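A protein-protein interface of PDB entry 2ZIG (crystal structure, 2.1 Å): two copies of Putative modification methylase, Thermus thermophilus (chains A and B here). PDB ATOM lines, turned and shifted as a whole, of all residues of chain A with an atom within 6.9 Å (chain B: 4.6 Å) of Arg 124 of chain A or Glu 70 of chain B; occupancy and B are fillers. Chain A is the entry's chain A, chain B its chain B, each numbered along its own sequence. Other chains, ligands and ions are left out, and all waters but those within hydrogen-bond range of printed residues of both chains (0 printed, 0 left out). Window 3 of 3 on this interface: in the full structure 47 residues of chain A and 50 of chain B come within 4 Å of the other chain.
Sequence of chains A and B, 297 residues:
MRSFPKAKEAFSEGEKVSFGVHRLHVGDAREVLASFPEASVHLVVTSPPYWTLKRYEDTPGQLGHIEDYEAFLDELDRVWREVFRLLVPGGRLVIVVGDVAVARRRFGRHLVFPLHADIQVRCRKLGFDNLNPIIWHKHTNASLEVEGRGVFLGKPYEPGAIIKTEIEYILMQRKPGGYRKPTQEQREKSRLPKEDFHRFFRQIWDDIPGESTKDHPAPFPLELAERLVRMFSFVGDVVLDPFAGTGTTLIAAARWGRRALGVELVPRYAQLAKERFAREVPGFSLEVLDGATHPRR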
ATOM      1  N   ILE A 119     -10.981  34.130 -26.798  1.00  0.00           N
ATOM      2  CA  ILE A 119      -9.932  33.695 -25.895  1.00  0.00           C
ATOM      3  C   ILE A 119     -10.471  32.633 -24.942  1.00  0.00           C
ATOM      4  O   ILE A 119      -9.814  31.624 -24.705  1.00  0.00           O
ATOM      5  CB  ILE A 119      -9.344  34.896 -25.125  1.00  0.00           C
ATOM      6  CG1 ILE A 119      -8.650  35.827 -26.123  1.00  0.00           C
ATOM      7  CG2 ILE A 119      -8.353  34.428 -24.058  1.00  0.00           C
ATOM      8  CD1 ILE A 119      -8.023  37.062 -25.508  1.00  0.00           C
ATOM      9  N   GLN A 120     -11.679  32.835 -24.418  1.00  0.00           N
ATOM     10  CA  GLN A 120     -12.249  31.850 -23.513  1.00  0.00           C
ATOM     11  C   GLN A 120     -12.427  30.509 -24.216  1.00  0.00           C
ATOM     12  O   GLN A 120     -12.033  29.462 -23.693  1.00  0.00           O
ATOM     13  CB  GLN A 120     -13.609  32.309 -22.982  1.00  0.00           C
ATOM     14  CG  GLN A 120     -13.563  33.470 -22.002  1.00  0.00           C
ATOM     15  CD  GLN A 120     -14.907  33.717 -21.347  1.00  0.00           C
ATOM     16  OE1 GLN A 120     -15.201  33.194 -20.264  1.00  0.00           O
ATOM     17  NE2 GLN A 120     -15.738  34.496 -22.010  1.00  0.00           N
ATOM     18  N   VAL A 121     -13.031  30.539 -25.398  1.00  0.00           N
ATOM     19  CA  VAL A 121     -13.261  29.302 -26.120  1.00  0.00           C
ATOM     20  C   VAL A 121     -11.961  28.584 -26.448  1.00  0.00           C
ATOM     21  O   VAL A 121     -11.865  27.372 -26.287  1.00  0.00           O
ATOM     22  CB  VAL A 121     -14.040  29.548 -27.404  1.00  0.00           C
ATOM     23  CG1 VAL A 121     -14.277  28.225 -28.116  1.00  0.00           C
ATOM     24  CG2 VAL A 121     -15.373  30.195 -27.080  1.00  0.00           C
ATOM     25  N   ARG A 122     -10.956  29.332 -26.888  1.00  0.00           N
ATOM     26  CA  ARG A 122      -9.672  28.738 -27.238  1.00  0.00           C
ATOM     27  C   ARG A 122      -8.924  28.209 -26.021  1.00  0.00           C
ATOM     28  O   ARG A 122      -8.200  27.223 -26.114  1.00  0.00           O
ATOM     29  CB  ARG A 122      -8.824  29.753 -28.005  1.00  0.00           C
ATOM     30  CG  ARG A 122      -9.468  30.109 -29.342  1.00  0.00           C
ATOM     31  CD  ARG A 122      -8.984  31.430 -29.885  1.00  0.00           C
ATOM     32  NE  ARG A 122      -7.897  31.260 -30.839  1.00  0.00           N
ATOM     33  CZ  ARG A 122      -8.019  30.646 -32.008  1.00  0.00           C
ATOM     34  NH1 ARG A 122      -9.185  30.141 -32.377  1.00  0.00           N
ATOM     35  NH2 ARG A 122      -6.973  30.541 -32.808  1.00  0.00           N
ATOM     36  N   CYS A 123      -9.096  28.850 -24.873  1.00  0.00           N
ATOM     37  CA  CYS A 123      -8.416  28.371 -23.676  1.00  0.00           C
ATOM     38  C   CYS A 123      -8.998  27.033 -23.230  1.00  0.00           C
ATOM     39  O   CYS A 123      -8.304  26.211 -22.636  1.00  0.00           O
ATOM     40  CB  CYS A 123      -8.524  29.399 -22.553  1.00  0.00           C
ATOM     41  SG  CYS A 123      -7.298  30.700 -22.667  1.00  0.00           S
ATOM     42  N   ARG A 124     -10.271  26.808 -23.526  1.00  0.00           N
ATOM     43  CA  ARG A 124     -10.902  25.551 -23.152  1.00  0.00           C
ATOM     44  C   ARG A 124     -10.212  24.434 -23.910  1.00  0.00           C
ATOM     45  O   ARG A 124      -9.911  23.378 -23.350  1.00  0.00           O
ATOM     46  CB  ARG A 124     -12.393  25.566 -23.491  1.00  0.00           C
ATOM     47  CG  ARG A 124     -13.099  24.246 -23.210  1.00  0.00           C
ATOM     48  CD  ARG A 124     -14.523  24.461 -22.695  1.00  0.00           C
ATOM     49  NE  ARG A 124     -15.317  25.325 -23.568  1.00  0.00           N
ATOM     50  CZ  ARG A 124     -15.576  25.063 -24.841  1.00  0.00           C
ATOM     51  NH1 ARG A 124     -15.111  23.956 -25.401  1.00  0.00           N
ATOM     52  NH2 ARG A 124     -16.296  25.907 -25.556  1.00  0.00           N
ATOM     53  N   LYS A 125      -9.944  24.673 -25.187  1.00  0.00           N
ATOM     54  CA  LYS A 125      -9.273  23.673 -26.003  1.00  0.00           C
ATOM     55  C   LYS A 125      -7.889  23.369 -25.426  1.00  0.00           C
ATOM     56  O   LYS A 125      -7.377  22.258 -25.562  1.00  0.00           O
ATOM     57  CB  LYS A 125      -9.136  24.167 -27.444  1.00  0.00           C
ATOM     58  CG  LYS A 125      -8.481  23.150 -28.365  1.00  0.00           C
ATOM     59  CD  LYS A 125      -8.456  23.621 -29.812  1.00  0.00           C
ATOM     60  CE  LYS A 125      -7.784  22.591 -30.710  1.00  0.00           C
ATOM     61  NZ  LYS A 125      -6.418  22.236 -30.216  1.00  0.00           N
ATOM     62  N   LEU A 126      -7.292  24.359 -24.769  1.00  0.00           N
ATOM     63  CA  LEU A 126      -5.966  24.192 -24.182  1.00  0.00           C
ATOM     64  C   LEU A 126      -5.966  23.417 -22.873  1.00  0.00           C
ATOM     65  O   LEU A 126      -4.906  23.133 -22.320  1.00  0.00           O
ATOM     66  CB  LEU A 126      -5.307  25.557 -23.973  1.00  0.00           C
ATOM     67  CG  LEU A 126      -4.641  26.194 -25.197  1.00  0.00           C
ATOM     68  CD1 LEU A 126      -5.492  25.992 -26.423  1.00  0.00           C
ATOM     69  CD2 LEU A 126      -4.405  27.674 -24.941  1.00  0.00           C
ATOM     70  N   GLY A 127      -7.148  23.080 -22.374  1.00  0.00           N
ATOM     71  CA  GLY A 127      -7.220  22.320 -21.135  1.00  0.00           C
ATOM     72  C   GLY A 127      -7.522  23.130 -19.886  1.00  0.00           C
ATOM     73  O   GLY A 127      -7.520  22.585 -18.783  1.00  0.00           O
ATOM     74  N   PHE A 128      -7.774  24.425 -20.051  1.00  0.00           N
ATOM     75  CA  PHE A 128      -8.083  25.294 -18.927  1.00  0.00           C
ATOM     76  C   PHE A 128      -9.522  25.100 -18.475  1.00  0.00           C
ATOM     77  O   PHE A 128     -10.399  24.745 -19.268  1.00  0.00           O
ATOM     78  CB  PHE A 128      -7.918  26.773 -19.309  1.00  0.00           C
ATOM     79  CG  PHE A 128      -6.491  27.257 -19.343  1.00  0.00           C
ATOM     80  CD1 PHE A 128      -5.816  27.557 -18.168  1.00  0.00           C
ATOM     81  CD2 PHE A 128      -5.841  27.456 -20.560  1.00  0.00           C
ATOM     82  CE1 PHE A 128      -4.518  28.053 -18.198  1.00  0.00           C
ATOM     83  CE2 PHE A 128      -4.543  27.950 -20.604  1.00  0.00           C
ATOM     84  CZ  PHE A 128      -3.878  28.250 -19.422  1.00  0.00           C
ATOM     85  N   ASP A 129      -9.757  25.338 -17.193  1.00  0.00           N
ATOM     86  CA  ASP A 129     -11.101  25.273 -16.642  1.00  0.00           C
ATOM     87  C   ASP A 129     -11.552  26.729 -16.655  1.00  0.00           C
ATOM     88  O   ASP A 129     -10.861  27.610 -16.145  1.00  0.00           O
ATOM     89  CB  ASP A 129     -11.091  24.759 -15.199  1.00  0.00           C
ATOM     90  CG  ASP A 129     -11.192  23.242 -15.109  1.00  0.00           C
ATOM     91  OD1 ASP A 129     -11.445  22.590 -16.150  1.00  0.00           O
ATOM     92  OD2 ASP A 129     -11.035  22.705 -13.989  1.00  0.00           O
ATOM     93  N   ASN A 130     -12.703  27.000 -17.241  1.00  0.00           N
ATOM     94  CA  ASN A 130     -13.157  28.373 -17.276  1.00  0.00           C
ATOM     95  C   ASN A 130     -13.932  28.727 -16.016  1.00  0.00           C
ATOM     96  O   ASN A 130     -14.750  27.948 -15.544  1.00  0.00           O
ATOM     97  CB  ASN A 130     -14.015  28.605 -18.518  1.00  0.00           C
ATOM     98  CG  ASN A 130     -14.680  29.954 -18.509  1.00  0.00           C
ATOM     99  OD1 ASN A 130     -15.768  30.117 -17.957  1.00  0.00           O
ATOM    100  ND2 ASN A 130     -14.021  30.943 -19.103  1.00  0.00           N
ATOM    101  N   GLN A 173      -8.998  31.713 -16.091  1.00  0.00           N
ATOM    102  CA  GLN A 173      -8.755  30.378 -16.635  1.00  0.00           C
ATOM    103  C   GLN A 173      -7.893  29.590 -15.663  1.00  0.00           C
ATOM    104  O   GLN A 173      -6.723  29.903 -15.442  1.00  0.00           O
ATOM    105  CB  GLN A 173      -8.069  30.508 -17.994  1.00  0.00           C
ATOM    106  CG  GLN A 173      -8.883  31.323 -18.987  1.00  0.00           C
ATOM    107  CD  GLN A 173     -10.225  30.676 -19.279  1.00  0.00           C
ATOM    108  OE1 GLN A 173     -11.280  31.288 -19.103  1.00  0.00           O
ATOM    109  NE2 GLN A 173     -10.192  29.433 -19.724  1.00  0.00           N
ATOM    110  N   ILE B  66     -18.155  17.693 -22.284  1.00  0.00           N
ATOM    111  CA  ILE B  66     -18.051  18.589 -23.430  1.00  0.00           C
ATOM    112  C   ILE B  66     -18.858  18.085 -24.623  1.00  0.00           C
ATOM    113  O   ILE B  66     -19.309  18.877 -25.449  1.00  0.00           O
ATOM    114  CB  ILE B  66     -16.576  18.803 -23.852  1.00  0.00           C
ATOM    115  CG1 ILE B  66     -15.847  19.617 -22.777  1.00  0.00           C
ATOM    116  CG2 ILE B  66     -16.506  19.527 -25.188  1.00  0.00           C
ATOM    117  CD1 ILE B  66     -14.451  20.064 -23.168  1.00  0.00           C
ATOM    118  N   GLU B  67     -19.046  16.771 -24.708  1.00  0.00           N
ATOM    119  CA  GLU B  67     -19.816  16.187 -25.803  1.00  0.00           C
ATOM    120  C   GLU B  67     -21.236  16.733 -25.800  1.00  0.00           C
ATOM    121  O   GLU B  67     -21.680  17.323 -26.780  1.00  0.00           O
ATOM    122  CB  GLU B  67     -19.857  14.655 -25.691  1.00  0.00           C
ATOM    123  CG  GLU B  67     -18.563  13.949 -26.082  1.00  0.00           C
ATOM    124  CD  GLU B  67     -18.162  14.202 -27.530  1.00  0.00           C
ATOM    125  OE1 GLU B  67     -17.154  13.613 -27.979  1.00  0.00           O
ATOM    126  OE2 GLU B  67     -18.850  14.989 -28.218  1.00  0.00           O
ATOM    127  N   ASP B  68     -21.943  16.530 -24.692  1.00  0.00           N
ATOM    128  CA  ASP B  68     -23.312  17.017 -24.567  1.00  0.00           C
ATOM    129  C   ASP B  68     -23.314  18.495 -24.911  1.00  0.00           C
ATOM    130  O   ASP B  68     -24.187  18.981 -25.627  1.00  0.00           O
ATOM    131  CB  ASP B  68     -23.823  16.844 -23.132  1.00  0.00           C
ATOM    132  CG  ASP B  68     -23.628  15.438 -22.606  1.00  0.00           C
ATOM    133  OD1 ASP B  68     -22.460  15.028 -22.423  1.00  0.00           O
ATOM    134  OD2 ASP B  68     -24.643  14.743 -22.376  1.00  0.00           O
ATOM    135  N   TYR B  69     -22.313  19.193 -24.385  1.00  0.00           N
ATOM    136  CA  TYR B  69     -22.140  20.622 -24.592  1.00  0.00           C
ATOM    137  C   TYR B  69     -21.981  20.967 -26.074  1.00  0.00           C
ATOM    138  O   TYR B  69     -22.712  21.807 -26.599  1.00  0.00           O
ATOM    139  CB  TYR B  69     -20.917  21.098 -23.800  1.00  0.00           C
ATOM    140  CG  TYR B  69     -20.750  22.596 -23.740  1.00  0.00           C
ATOM    141  CD1 TYR B  69     -21.734  23.405 -23.173  1.00  0.00           C
ATOM    142  CD2 TYR B  69     -19.615  23.208 -24.263  1.00  0.00           C
ATOM    143  CE1 TYR B  69     -21.592  24.787 -23.135  1.00  0.00           C
ATOM    144  CE2 TYR B  69     -19.461  24.588 -24.230  1.00  0.00           C
ATOM    145  CZ  TYR B  69     -20.454  25.371 -23.666  1.00  0.00           C
ATOM    146  OH  TYR B  69     -20.308  26.739 -23.641  1.00  0.00           O
ATOM    147  N   GLU B  70     -21.034  20.315 -26.746  1.00  0.00           N
ATOM    148  CA  GLU B  70     -20.797  20.569 -28.169  1.00  0.00           C
ATOM    149  C   GLU B  70     -22.036  20.268 -29.005  1.00  0.00           C
ATOM    150  O   GLU B  70     -22.408  21.048 -29.887  1.00  0.00           O
ATOM    151  CB  GLU B  70     -19.631  19.728 -28.697  1.00  0.00           C
ATOM    152  CG  GLU B  70     -18.320  19.907 -27.957  1.00  0.00           C
ATOM    153  CD  GLU B  70     -17.951  21.361 -27.747  1.00  0.00           C
ATOM    154  OE1 GLU B  70     -17.863  22.110 -28.747  1.00  0.00           O
ATOM    155  OE2 GLU B  70     -17.745  21.752 -26.578  1.00  0.00           O
ATOM    156  N   ALA B  71     -22.665  19.130 -28.732  1.00  0.00           N
ATOM    157  CA  ALA B  71     -23.865  18.735 -29.461  1.00  0.00           C
ATOM    158  C   ALA B  71     -24.969  19.780 -29.255  1.00  0.00           C
ATOM    159  O   ALA B  71     -25.720  20.095 -30.178  1.00  0.00           O
ATOM    160  CB  ALA B  71     -24.332  17.368 -28.988  1.00  0.00           C
ATOM    161  N   PHE B  72     -25.063  20.311 -28.041  1.00  0.00           N
ATOM    162  CA  PHE B  72     -26.057  21.329 -27.729  1.00  0.00           C
ATOM    163  C   PHE B  72     -25.753  22.567 -28.568  1.00  0.00           C
ATOM    164  O   PHE B  72     -26.631  23.115 -29.227  1.00  0.00           O
ATOM    165  CB  PHE B  72     -26.007  21.674 -26.236  1.00  0.00           C
ATOM    166  CG  PHE B  72     -26.988  22.736 -25.825  1.00  0.00           C
ATOM    167  CD1 PHE B  72     -28.351  22.578 -26.066  1.00  0.00           C
ATOM    168  CD2 PHE B  72     -26.549  23.898 -25.201  1.00  0.00           C
ATOM    169  CE1 PHE B  72     -29.265  23.569 -25.692  1.00  0.00           C
ATOM    170  CE2 PHE B  72     -27.457  24.897 -24.822  1.00  0.00           C
ATOM    171  CZ  PHE B  72     -28.815  24.731 -25.068  1.00  0.00           C
ATOM    172  N   LEU B  73     -24.498  23.000 -28.549  1.00  0.00           N
ATOM    173  CA  LEU B  73     -24.086  24.162 -29.328  1.00  0.00           C
ATOM    174  C   LEU B  73     -24.444  23.978 -30.798  1.00  0.00           C
ATOM    175  O   LEU B  73     -24.947  24.897 -31.448  1.00  0.00           O
ATOM    176  CB  LEU B  73     -22.582  24.381 -29.189  1.00  0.00           C
ATOM    177  CG  LEU B  73     -22.131  24.931 -27.837  1.00  0.00           C
ATOM    178  CD1 LEU B  73     -20.617  24.990 -27.781  1.00  0.00           C
ATOM    179  CD2 LEU B  73     -22.735  26.319 -27.643  1.00  0.00           C
ATOM    180  N   ASP B  74     -24.187  22.778 -31.312  1.00  0.00           N
ATOM    181  CA  ASP B  74     -24.477  22.456 -32.704  1.00  0.00           C
ATOM    182  C   ASP B  74     -25.970  22.556 -32.984  1.00  0.00           C
ATOM    183  O   ASP B  74     -26.379  22.952 -34.074  1.00  0.00           O
ATOM    184  CB  ASP B  74     -23.960  21.049 -33.032  1.00  0.00           C
ATOM    185  CG  ASP B  74     -22.445  21.006 -33.186  1.00  0.00           C
ATOM    186  OD1 ASP B  74     -21.865  19.904 -33.087  1.00  0.00           O
ATOM    187  OD2 ASP B  74     -21.832  22.075 -33.418  1.00  0.00           O
ATOM    188  N   PRO B 114     -18.507  28.483 -20.619  1.00  0.00           N
ATOM    189  CA  PRO B 114     -18.636  29.831 -21.196  1.00  0.00           C
ATOM    190  C   PRO B 114     -19.645  29.886 -22.348  1.00  0.00           C
ATOM    191  O   PRO B 114     -19.304  30.264 -23.469  1.00  0.00           O
ATOM    192  CB  PRO B 114     -17.216  30.135 -21.660  1.00  0.00           C
ATOM    193  CG  PRO B 114     -16.747  28.791 -22.140  1.00  0.00           C
ATOM    194  CD  PRO B 114     -17.242  27.850 -21.043  1.00  0.00           C
ATOM    195  N   ASP B 118     -19.148  30.812 -26.433  1.00  0.00           N
ATOM    196  CA  ASP B 118     -19.256  29.797 -27.472  1.00  0.00           C
ATOM    197  C   ASP B 118     -20.293  30.243 -28.488  1.00  0.00           C
ATOM    198  O   ASP B 118     -20.121  30.039 -29.691  1.00  0.00           O
ATOM    199  CB  ASP B 118     -19.656  28.443 -26.866  1.00  0.00           C
ATOM    200  CG  ASP B 118     -18.458  27.671 -26.332  1.00  0.00           C
ATOM    201  OD1 ASP B 118     -17.540  27.403 -27.134  1.00  0.00           O
ATOM    202  OD2 ASP B 118     -18.425  27.339 -25.127  1.00  0.00           O
ATOM    203  N   ARG B 122     -19.432  31.020 -32.506  1.00  0.00           N
ATOM    204  CA  ARG B 122     -20.141  30.269 -33.528  1.00  0.00           C
ATOM    205  C   ARG B 122     -21.026  31.135 -34.424  1.00  0.00           C
ATOM    206  O   ARG B 122     -21.227  30.808 -35.593  1.00  0.00           O
ATOM    207  CB  ARG B 122     -20.956  29.159 -32.870  1.00  0.00           C
ATOM    208  CG  ARG B 122     -20.091  28.050 -32.298  1.00  0.00           C
ATOM    209  CD  ARG B 122     -20.885  27.150 -31.379  1.00  0.00           C
ATOM    210  NE  ARG B 122     -20.146  25.946 -31.002  1.00  0.00           N
ATOM    211  CZ  ARG B 122     -20.191  24.798 -31.672  1.00  0.00           C
ATOM    212  NH1 ARG B 122     -20.944  24.689 -32.760  1.00  0.00           N
ATOM    213  NH2 ARG B 122     -19.491  23.753 -31.251  1.00  0.00           N
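Of the printed residues of chain B, Arg 124 of chain A touches Tyr 69 (3.7 Å), Glu 70 (3.6 Å) and Asp 118 (2.5 Å). Glu 70 of chain B touches just one residue of chain A: Arg 124. Of the printed residues of chain B, Val 121 of chain A touches Asp 118. Printed residues of chain A within 4 Å of Asp 118 of chain B: Val 121 and Arg 124. Printed residues of chain A within 4 Å of Pro 114 of chain B: Gln 120 (3.9 Å) and Asn 130 (3.98 Å). Of the printed residues of chain B, Gln 120 of chain A touches Pro 114. The nearest printed residue of chain B that does not touch Arg 124 of chain A is Pro 114 of chain B (4.01 Å).
OE1 of Gln 120 of chain A touches CB of Pro 114 of chain B, at 3.9 Å. Val 121 of chain A touches Asp 118 of chain B. Tyr 69 of chain B touches Arg 124 of chain A. Asn 130 of chain A touches Pro 114 of chain B (OD1 to CB, 3.98 Å).
1 position is printed for both chains. Of the 6 pairs that touch across the chains among the printed residues, none has its exchanged pair printed and touching as well.
ND2 of Asn 130 of chain A is in hydrogen-bond range of OE1 of Gln 173 of chain A (2.8 Å). OE1 of Gln 120 of chain A lies within hydrogen-bond range of ND2 of Asn 130 of chain A (2.8 Å). The side-chain carboxylate (OE1) of Glu 70 of chain B lies within salt-bridge range of the guanidinium group (NH2) of Arg 122 of chain B, 3.4 Å away. OD2 of Asp 118 of chain B is in hydrogen-bond range of OH of Tyr 69 of chain B (2.5 Å).
The guanidinium group (NH1) of Arg 124 of chain A is in salt-bridge range of the side-chain carboxylate (OE2) of Glu 70 of chain B. The guanidinium group (NH2) of Arg 124 of chain A is in salt-bridge range of the side-chain carboxylate (OD1) of Asp 118 of chain B (2.5 Å).
Of the 12 printed residues of chain B, 4 touch a printed residue of chain A. Hydrophobic or aromatic side chains of chain A within 4 Å of the printed part of chain B: Val 121. Among the printed residues, Asp or Glu carboxylates within 4 Å of a Lys or Arg side-chain nitrogen of the other chain: Arg 124 of chain A with Glu 70 of chain B (3.6 Å) and Arg 124 of chain A with Asp 118 of chain B (2.5 Å).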
